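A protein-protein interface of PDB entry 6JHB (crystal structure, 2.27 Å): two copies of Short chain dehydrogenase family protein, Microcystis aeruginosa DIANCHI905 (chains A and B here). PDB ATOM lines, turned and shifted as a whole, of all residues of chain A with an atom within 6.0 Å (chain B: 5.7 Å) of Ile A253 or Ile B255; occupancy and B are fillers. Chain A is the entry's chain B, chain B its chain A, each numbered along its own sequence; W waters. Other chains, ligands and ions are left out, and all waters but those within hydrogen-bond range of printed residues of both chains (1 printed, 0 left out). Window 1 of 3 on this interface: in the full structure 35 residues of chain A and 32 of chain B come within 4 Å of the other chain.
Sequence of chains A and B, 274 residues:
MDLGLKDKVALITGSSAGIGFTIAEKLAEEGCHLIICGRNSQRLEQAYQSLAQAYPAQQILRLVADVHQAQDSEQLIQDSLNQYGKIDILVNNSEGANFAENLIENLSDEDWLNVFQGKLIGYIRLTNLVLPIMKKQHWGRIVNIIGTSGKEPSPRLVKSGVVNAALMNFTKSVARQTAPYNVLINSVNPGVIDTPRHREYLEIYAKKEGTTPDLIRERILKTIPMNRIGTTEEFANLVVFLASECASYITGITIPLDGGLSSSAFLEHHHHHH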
ATOM      1  N   THR A 171      33.116  -4.983  -3.814  1.00  0.00           N
ATOM      2  CA  THR A 171      31.831  -4.564  -4.361  1.00  0.00           C
ATOM      3  C   THR A 171      30.787  -4.542  -3.249  1.00  0.00           C
ATOM      4  O   THR A 171      30.107  -3.547  -3.036  1.00  0.00           O
ATOM      5  CB  THR A 171      31.384  -5.512  -5.504  1.00  0.00           C
ATOM      6  OG1 THR A 171      32.255  -5.338  -6.637  1.00  0.00           O
ATOM      7  CG2 THR A 171      29.934  -5.263  -5.943  1.00  0.00           C
ATOM      8  N   LYS A 172      30.681  -5.645  -2.530  1.00  0.00           N
ATOM      9  CA  LYS A 172      29.672  -5.762  -1.479  1.00  0.00           C
ATOM     10  C   LYS A 172      29.853  -4.698  -0.410  1.00  0.00           C
ATOM     11  O   LYS A 172      28.878  -4.108   0.053  1.00  0.00           O
ATOM     12  CB  LYS A 172      29.723  -7.135  -0.813  1.00  0.00           C
ATOM     13  CG  LYS A 172      29.421  -8.292  -1.739  1.00  0.00           C
ATOM     14  CD  LYS A 172      29.149  -9.552  -0.925  1.00  0.00           C
ATOM     15  N   ALA A 175      29.118  -1.091  -1.681  1.00  0.00           N
ATOM     16  CA  ALA A 175      27.702  -0.940  -1.972  1.00  0.00           C
ATOM     17  C   ALA A 175      26.924  -0.684  -0.702  1.00  0.00           C
ATOM     18  O   ALA A 175      26.036   0.167  -0.664  1.00  0.00           O
ATOM     19  CB  ALA A 175      27.164  -2.189  -2.635  1.00  0.00           C
ATOM     20  N   ILE A 185      26.501   0.061  -6.686  1.00  0.00           N
ATOM     21  CA  ILE A 185      27.737  -0.555  -7.143  1.00  0.00           C
ATOM     22  C   ILE A 185      27.499  -2.027  -7.383  1.00  0.00           C
ATOM     23  O   ILE A 185      27.090  -2.734  -6.490  1.00  0.00           O
ATOM     24  CB  ILE A 185      28.824  -0.359  -6.097  1.00  0.00           C
ATOM     25  CG1 ILE A 185      28.727   1.080  -5.559  1.00  0.00           C
ATOM     26  CG2 ILE A 185      30.176  -0.753  -6.663  1.00  0.00           C
ATOM     27  CD1 ILE A 185      30.015   1.866  -5.557  1.00  0.00           C
ATOM     28  N   ASN A 186      27.734  -2.478  -8.602  1.00  0.00           N
ATOM     29  CA  ASN A 186      27.594  -3.876  -8.911  1.00  0.00           C
ATOM     30  C   ASN A 186      28.738  -4.334  -9.767  1.00  0.00           C
ATOM     31  O   ASN A 186      29.593  -3.539 -10.183  1.00  0.00           O
ATOM     32  CB  ASN A 186      26.264  -4.171  -9.581  1.00  0.00           C
ATOM     33  CG  ASN A 186      25.100  -3.802  -8.714  1.00  0.00           C
ATOM     34  OD1 ASN A 186      24.830  -4.458  -7.708  1.00  0.00           O
ATOM     35  ND2 ASN A 186      24.411  -2.738  -9.075  1.00  0.00           N
ATOM     36  N   SER A 187      28.779  -5.633  -9.983  1.00  0.00           N
ATOM     37  CA  SER A 187      29.808  -6.214 -10.815  1.00  0.00           C
ATOM     38  C   SER A 187      29.215  -7.229 -11.774  1.00  0.00           C
ATOM     39  O   SER A 187      28.159  -7.820 -11.503  1.00  0.00           O
ATOM     40  CB  SER A 187      30.844  -6.854  -9.922  1.00  0.00           C
ATOM     41  OG  SER A 187      31.522  -5.830  -9.210  1.00  0.00           O
ATOM     42  N   VAL A 188      29.885  -7.387 -12.902  1.00  0.00           N
ATOM     43  CA  VAL A 188      29.501  -8.340 -13.932  1.00  0.00           C
ATOM     44  C   VAL A 188      30.702  -9.228 -14.213  1.00  0.00           C
ATOM     45  O   VAL A 188      31.828  -8.751 -14.391  1.00  0.00           O
ATOM     46  CB  VAL A 188      29.048  -7.640 -15.229  1.00  0.00           C
ATOM     47  CG1 VAL A 188      28.552  -8.626 -16.263  1.00  0.00           C
ATOM     48  CG2 VAL A 188      27.946  -6.654 -14.936  1.00  0.00           C
ATOM     49  N   LEU A 242      22.238  -2.154 -15.629  1.00  0.00           N
ATOM     50  CA  LEU A 242      22.696  -1.851 -14.283  1.00  0.00           C
ATOM     51  C   LEU A 242      23.102  -0.409 -14.113  1.00  0.00           C
ATOM     52  O   LEU A 242      23.081   0.097 -12.996  1.00  0.00           O
ATOM     53  CB  LEU A 242      23.878  -2.723 -13.909  1.00  0.00           C
ATOM     54  CG  LEU A 242      23.522  -4.185 -13.659  1.00  0.00           C
ATOM     55  CD1 LEU A 242      24.825  -4.972 -13.688  1.00  0.00           C
ATOM     56  CD2 LEU A 242      22.767  -4.348 -12.349  1.00  0.00           C
ATOM     57  N   ILE A 250      19.016  -2.321  -7.158  1.00  0.00           N
ATOM     58  CA  ILE A 250      20.001  -3.390  -7.240  1.00  0.00           C
ATOM     59  C   ILE A 250      21.346  -2.847  -6.821  1.00  0.00           C
ATOM     60  O   ILE A 250      21.911  -1.992  -7.489  1.00  0.00           O
ATOM     61  CB  ILE A 250      20.128  -3.967  -8.657  1.00  0.00           C
ATOM     62  CG1 ILE A 250      18.796  -4.578  -9.107  1.00  0.00           C
ATOM     63  CG2 ILE A 250      21.177  -5.081  -8.690  1.00  0.00           C
ATOM     64  CD1 ILE A 250      18.683  -4.708 -10.605  1.00  0.00           C
ATOM     65  N   THR A 251      21.879  -3.341  -5.722  1.00  0.00           N
ATOM     66  CA  THR A 251      23.235  -2.988  -5.383  1.00  0.00           C
ATOM     67  C   THR A 251      23.953  -4.123  -4.616  1.00  0.00           C
ATOM     68  O   THR A 251      23.327  -4.974  -4.015  1.00  0.00           O
ATOM     69  CB  THR A 251      23.269  -1.628  -4.667  1.00  0.00           C
ATOM     70  OG1 THR A 251      24.584  -1.076  -4.780  1.00  0.00           O
ATOM     71  CG2 THR A 251      22.848  -1.730  -3.220  1.00  0.00           C
ATOM     72  N   GLY A 252      25.269  -4.135  -4.709  1.00  0.00           N
ATOM     73  CA  GLY A 252      26.111  -5.100  -4.001  1.00  0.00           C
ATOM     74  C   GLY A 252      26.228  -6.493  -4.611  1.00  0.00           C
ATOM     75  O   GLY A 252      26.730  -7.414  -3.984  1.00  0.00           O
ATOM     76  N   ILE A 253      25.790  -6.660  -5.843  1.00  0.00           N
ATOM     77  CA  ILE A 253      25.736  -7.991  -6.375  1.00  0.00           C
ATOM     78  C   ILE A 253      26.714  -8.078  -7.510  1.00  0.00           C
ATOM     79  O   ILE A 253      27.053  -7.056  -8.121  1.00  0.00           O
ATOM     80  CB  ILE A 253      24.312  -8.392  -6.824  1.00  0.00           C
ATOM     81  CG1 ILE A 253      23.819  -7.497  -7.957  1.00  0.00           C
ATOM     82  CG2 ILE A 253      23.343  -8.304  -5.649  1.00  0.00           C
ATOM     83  CD1 ILE A 253      22.793  -8.170  -8.828  1.00  0.00           C
ATOM     84  N   THR A 254      27.167  -9.299  -7.759  1.00  0.00           N
ATOM     85  CA  THR A 254      27.961  -9.615  -8.915  1.00  0.00           C
ATOM     86  C   THR A 254      27.178 -10.650  -9.702  1.00  0.00           C
ATOM     87  O   THR A 254      26.790 -11.665  -9.138  1.00  0.00           O
ATOM     88  CB  THR A 254      29.339 -10.163  -8.513  1.00  0.00           C
ATOM     89  OG1 THR A 254      30.013  -9.180  -7.712  1.00  0.00           O
ATOM     90  CG2 THR A 254      30.200 -10.450  -9.753  1.00  0.00           C
ATOM     91  N   ILE A 255      26.976 -10.380 -10.996  1.00  0.00           N
ATOM     92  CA  ILE A 255      26.216 -11.236 -11.924  1.00  0.00           C
ATOM     93  C   ILE A 255      27.095 -11.928 -12.979  1.00  0.00           C
ATOM     94  O   ILE A 255      27.838 -11.268 -13.695  1.00  0.00           O
ATOM     95  CB  ILE A 255      25.204 -10.390 -12.709  1.00  0.00           C
ATOM     96  CG1 ILE A 255      24.376  -9.539 -11.745  1.00  0.00           C
ATOM     97  CG2 ILE A 255      24.294 -11.283 -13.536  1.00  0.00           C
ATOM     98  CD1 ILE A 255      23.417  -8.580 -12.430  1.00  0.00           C
ATOM     99  N   SER B 187      16.530 -16.821 -11.998  1.00  0.00           N
ATOM    100  CA  SER B 187      15.705 -16.524 -10.856  1.00  0.00           C
ATOM    101  C   SER B 187      16.036 -15.154 -10.271  1.00  0.00           C
ATOM    102  O   SER B 187      17.158 -14.651 -10.415  1.00  0.00           O
ATOM    103  CB  SER B 187      15.860 -17.619  -9.801  1.00  0.00           C
ATOM    104  OG  SER B 187      15.410 -18.875 -10.323  1.00  0.00           O
ATOM    105  N   VAL B 188      15.037 -14.568  -9.623  1.00  0.00           N
ATOM    106  CA  VAL B 188      15.172 -13.275  -8.993  1.00  0.00           C
ATOM    107  C   VAL B 188      14.724 -13.411  -7.540  1.00  0.00           C
ATOM    108  O   VAL B 188      13.644 -13.930  -7.235  1.00  0.00           O
ATOM    109  CB  VAL B 188      14.324 -12.190  -9.685  1.00  0.00           C
ATOM    110  CG1 VAL B 188      14.546 -10.858  -8.993  1.00  0.00           C
ATOM    111  CG2 VAL B 188      14.663 -12.094 -11.164  1.00  0.00           C
ATOM    112  N   ASN B 189      15.559 -12.915  -6.651  1.00  0.00           N
ATOM    113  CA  ASN B 189      15.258 -12.916  -5.235  1.00  0.00           C
ATOM    114  C   ASN B 189      14.856 -11.563  -4.705  1.00  0.00           C
ATOM    115  O   ASN B 189      15.699 -10.701  -4.549  1.00  0.00           O
ATOM    116  CB  ASN B 189      16.475 -13.382  -4.474  1.00  0.00           C
ATOM    117  CG  ASN B 189      16.272 -14.708  -3.874  1.00  0.00           C
ATOM    118  OD1 ASN B 189      16.561 -15.732  -4.514  1.00  0.00           O
ATOM    119  ND2 ASN B 189      15.722 -14.728  -2.643  1.00  0.00           N
ATOM    120  N   PRO B 190      13.573 -11.376  -4.382  1.00  0.00           N
ATOM    121  CA  PRO B 190      13.225 -10.100  -3.796  1.00  0.00           C
ATOM    122  C   PRO B 190      13.777  -9.961  -2.379  1.00  0.00           C
ATOM    123  O   PRO B 190      13.905 -10.941  -1.677  1.00  0.00           O
ATOM    124  CB  PRO B 190      11.698 -10.116  -3.770  1.00  0.00           C
ATOM    125  CG  PRO B 190      11.276 -11.475  -4.176  1.00  0.00           C
ATOM    126  CD  PRO B 190      12.470 -12.342  -4.317  1.00  0.00           C
ATOM    127  N   LEU B 238      13.849  -5.616 -13.631  1.00  0.00           N
ATOM    128  CA  LEU B 238      14.823  -6.679 -13.770  1.00  0.00           C
ATOM    129  C   LEU B 238      14.252  -7.927 -14.448  1.00  0.00           C
ATOM    130  O   LEU B 238      14.889  -8.511 -15.325  1.00  0.00           O
ATOM    131  CB  LEU B 238      15.389  -7.061 -12.393  1.00  0.00           C
ATOM    132  CG  LEU B 238      16.392  -8.228 -12.436  1.00  0.00           C
ATOM    133  CD1 LEU B 238      17.487  -7.989 -13.478  1.00  0.00           C
ATOM    134  CD2 LEU B 238      17.052  -8.493 -11.091  1.00  0.00           C
ATOM    135  N   LEU B 242      15.392  -9.756 -17.911  1.00  0.00           N
ATOM    136  CA  LEU B 242      15.742 -11.174 -18.029  1.00  0.00           C
ATOM    137  C   LEU B 242      14.862 -11.883 -19.028  1.00  0.00           C
ATOM    138  O   LEU B 242      15.294 -12.854 -19.660  1.00  0.00           O
ATOM    139  CB  LEU B 242      15.618 -11.881 -16.692  1.00  0.00           C
ATOM    140  CG  LEU B 242      16.706 -11.498 -15.681  1.00  0.00           C
ATOM    141  CD1 LEU B 242      16.340 -12.069 -14.318  1.00  0.00           C
ATOM    142  CD2 LEU B 242      18.097 -11.941 -16.131  1.00  0.00           C
ATOM    143  N   ILE B 250      22.470 -14.764 -20.832  1.00  0.00           N
ATOM    144  CA  ILE B 250      22.305 -14.946 -19.400  1.00  0.00           C
ATOM    145  C   ILE B 250      21.404 -16.121 -19.102  1.00  0.00           C
ATOM    146  O   ILE B 250      20.210 -16.120 -19.413  1.00  0.00           O
ATOM    147  CB  ILE B 250      21.667 -13.712 -18.746  1.00  0.00           C
ATOM    148  CG1 ILE B 250      22.389 -12.451 -19.224  1.00  0.00           C
ATOM    149  CG2 ILE B 250      21.725 -13.841 -17.238  1.00  0.00           C
ATOM    150  CD1 ILE B 250      21.885 -11.157 -18.622  1.00  0.00           C
ATOM    151  N   ILE B 253      21.258 -18.313 -13.427  1.00  0.00           N
ATOM    152  CA  ILE B 253      21.674 -17.509 -12.313  1.00  0.00           C
ATOM    153  C   ILE B 253      20.488 -17.062 -11.491  1.00  0.00           C
ATOM    154  O   ILE B 253      19.382 -16.997 -11.977  1.00  0.00           O
ATOM    155  CB  ILE B 253      22.460 -16.284 -12.786  1.00  0.00           C
ATOM    156  CG1 ILE B 253      21.628 -15.460 -13.747  1.00  0.00           C
ATOM    157  CG2 ILE B 253      23.731 -16.750 -13.477  1.00  0.00           C
ATOM    158  CD1 ILE B 253      22.143 -14.077 -13.973  1.00  0.00           C
ATOM    159  N   THR B 254      20.747 -16.765 -10.228  1.00  0.00           N
ATOM    160  CA  THR B 254      19.753 -16.205  -9.348  1.00  0.00           C
ATOM    161  C   THR B 254      20.267 -14.845  -8.923  1.00  0.00           C
ATOM    162  O   THR B 254      21.383 -14.748  -8.429  1.00  0.00           O
ATOM    163  CB  THR B 254      19.530 -17.100  -8.123  1.00  0.00           C
ATOM    164  OG1 THR B 254      19.153 -18.409  -8.558  1.00  0.00           O
ATOM    165  CG2 THR B 254      18.417 -16.545  -7.235  1.00  0.00           C
ATOM    166  N   ILE B 255      19.462 -13.801  -9.132  1.00  0.00           N
ATOM    167  CA  ILE B 255      19.876 -12.436  -8.830  1.00  0.00           C
ATOM    168  C   ILE B 255      19.085 -11.821  -7.671  1.00  0.00           C
ATOM    169  O   ILE B 255      17.868 -11.780  -7.722  1.00  0.00           O
ATOM    170  CB  ILE B 255      19.698 -11.541 -10.059  1.00  0.00           C
ATOM    171  CG1 ILE B 255      20.623 -12.016 -11.186  1.00  0.00           C
ATOM    172  CG2 ILE B 255      20.024 -10.093  -9.709  1.00  0.00           C
ATOM    173  CD1 ILE B 255      20.189 -11.544 -12.547  1.00  0.00           C
ATOM    174  N   PRO B 256      19.776 -11.306  -6.634  1.00  0.00           N
ATOM    175  CA  PRO B 256      19.047 -10.636  -5.570  1.00  0.00           C
ATOM    176  C   PRO B 256      18.649  -9.232  -5.992  1.00  0.00           C
ATOM    177  O   PRO B 256      19.417  -8.532  -6.638  1.00  0.00           O
ATOM    178  CB  PRO B 256      20.056 -10.574  -4.418  1.00  0.00           C
ATOM    179  CG  PRO B 256      21.161 -11.498  -4.806  1.00  0.00           C
ATOM    180  CD  PRO B 256      21.200 -11.448  -6.298  1.00  0.00           C
ATOM    181  N   LEU B 257      17.446  -8.838  -5.613  1.00  0.00           N
ATOM    182  CA  LEU B 257      16.915  -7.541  -5.930  1.00  0.00           C
ATOM    183  C   LEU B 257      16.421  -7.025  -4.626  1.00  0.00           C
ATOM    184  O   LEU B 257      15.244  -7.232  -4.267  1.00  0.00           O
ATOM    185  CB  LEU B 257      15.773  -7.705  -6.915  1.00  0.00           C
ATOM    186  CG  LEU B 257      15.544  -6.498  -7.791  1.00  0.00           C
ATOM    187  CD1 LEU B 257      14.801  -6.965  -9.023  1.00  0.00           C
ATOM    188  CD2 LEU B 257      14.780  -5.411  -7.049  1.00  0.00           C
ATOM    189  N   ASP B 258      17.307  -6.387  -3.876  1.00  0.00           N
ATOM    190  CA  ASP B 258      17.059  -6.286  -2.447  1.00  0.00           C
ATOM    191  C   ASP B 258      17.512  -5.009  -1.756  1.00  0.00           C
ATOM    192  O   ASP B 258      17.558  -4.951  -0.514  1.00  0.00           O
ATOM    193  CB  ASP B 258      17.713  -7.495  -1.773  1.00  0.00           C
ATOM    194  CG  ASP B 258      19.233  -7.507  -1.939  1.00  0.00           C
ATOM    195  OD1 ASP B 258      19.874  -8.478  -1.484  1.00  0.00           O
ATOM    196  OD2 ASP B 258      19.791  -6.550  -2.514  1.00  0.00           O
ATOM    197  N   SER B 262      21.567  -8.315   0.780  1.00  0.00           N
ATOM    198  CA  SER B 262      22.620  -9.333   0.669  1.00  0.00           C
ATOM    199  C   SER B 262      24.055  -8.773   0.769  1.00  0.00           C
ATOM    200  O   SER B 262      24.995  -9.494   0.489  1.00  0.00           O
ATOM    201  CB  SER B 262      22.454 -10.162  -0.623  1.00  0.00           C
ATOM    202  OG  SER B 262      22.837  -9.416  -1.764  1.00  0.00           O
ATOM    203  N   SER B 263      24.231  -7.511   1.149  1.00  0.00           N
ATOM    204  CA  SER B 263      25.550  -7.028   1.592  1.00  0.00           C
ATOM    205  C   SER B 263      25.595  -6.971   3.114  1.00  0.00           C
ATOM    206  O   SER B 263      24.562  -6.792   3.755  1.00  0.00           O
ATOM    207  CB  SER B 263      25.849  -5.642   1.032  1.00  0.00           C
ATOM    208  OG  SER B 263      25.896  -5.658  -0.377  1.00  0.00           O
HETATM  209  O   HOH W   1      20.187  -6.035  -5.156  1.00  0.00           O
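The side-chain hydroxyl (OG) of Ser B263 sits at hydrogen-bond distance from the backbone carbonyl oxygen (O) of Lys A172.
The backbone carbonyl oxygen of Ile B253 sits at hydrogen-bond distance from the backbone NH of Ser B187 (2.9 Å).
The backbone carbonyl oxygen of Ser B187 sits at hydrogen-bond distance from the backbone NH of Ile B255 (2.8 Å).
The backbone NH (N) of Gly A252 lies within hydrogen-bond range of the backbone carbonyl oxygen (O) of Ile A185.
The side-chain amide oxygen (OD1) of Asn A186 is in hydrogen-bond range of the backbone NH (N) of Ile A253, at 3.0 Å.
The backbone NH of Ser A187 lies within hydrogen-bond range of the backbone carbonyl oxygen of Ile A253, at 2.9 Å.
The backbone carbonyl oxygen of Ser A187 is in hydrogen-bond range of the backbone NH of Ile A255 (2.9 Å).
Among the printed residues, merely in contact across the chains: Ile A250 with Leu B257 (3.999 Å), Gly A252 with Ser B263 (3.7 Å), Ile A253 with Ile B255 (3.5 Å), Ile A253 with Pro B256 (3.9 Å) and Ile A255 with Ile B253 (3.6 Å).
Val A188 touches none of the printed residues of chain B.
Leu A242 touches none of the printed residues of chain B.
Ile A253 touches just these residues of chain B: Ile B255 (3.5 Å) and Pro B256 (3.9 Å).
Of the printed residues of chain B, Ile A255 touches Ile B253.
Printed residues of chain A within 4 Å of Ile B253: Ile A255.
Printed residues of chain A within 4 Å of Leu B257: Ile A250 (3.999 Å).
The nearest residue of chain B that does not touch Ile A253 is Ser B262 (4.1 Å).
The nearest printed residue of chain A that does not touch Ile B253 is Thr A254 (7.1 Å).
Of the 14 printed residues of chain A, 5 touch a printed residue of chain B.
Printed residues of chain A that touch a printed residue of chain B: Lys A172, Ile A250, Gly A252, Ile A253 and Ile A255.
Hydrophobic or aromatic side chains of chain A within 4 Å of the printed part of chain B: Ile A250, Ile A253 and Ile A255.
Printed residues of chain B that touch a printed residue of chain A: Ile B253, Ile B255, Pro B256, Leu B257 and Ser B263.
Hydrophobic or aromatic side chains of chain B that line the printed part of chain A: Ile B253, Ile B255, Pro B256 and Leu B257.
Among the printed residues, no Asp or Glu carboxylate lies within 4 Å of a Lys or Arg side-chain nitrogen of the other chain.
Ile A253 touches Ile B255, and with the chains exchanged Ile A255 touches Ile B253.
Positions printed for both chains: 187, 188, 242, 250, 253, 254 and 255.
Water W1 lies within hydrogen-bond range of OD2 of Asp B258 (2.7 Å), O of Pro B256 (3.0 Å) and N of Thr A251 (3.2 Å).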
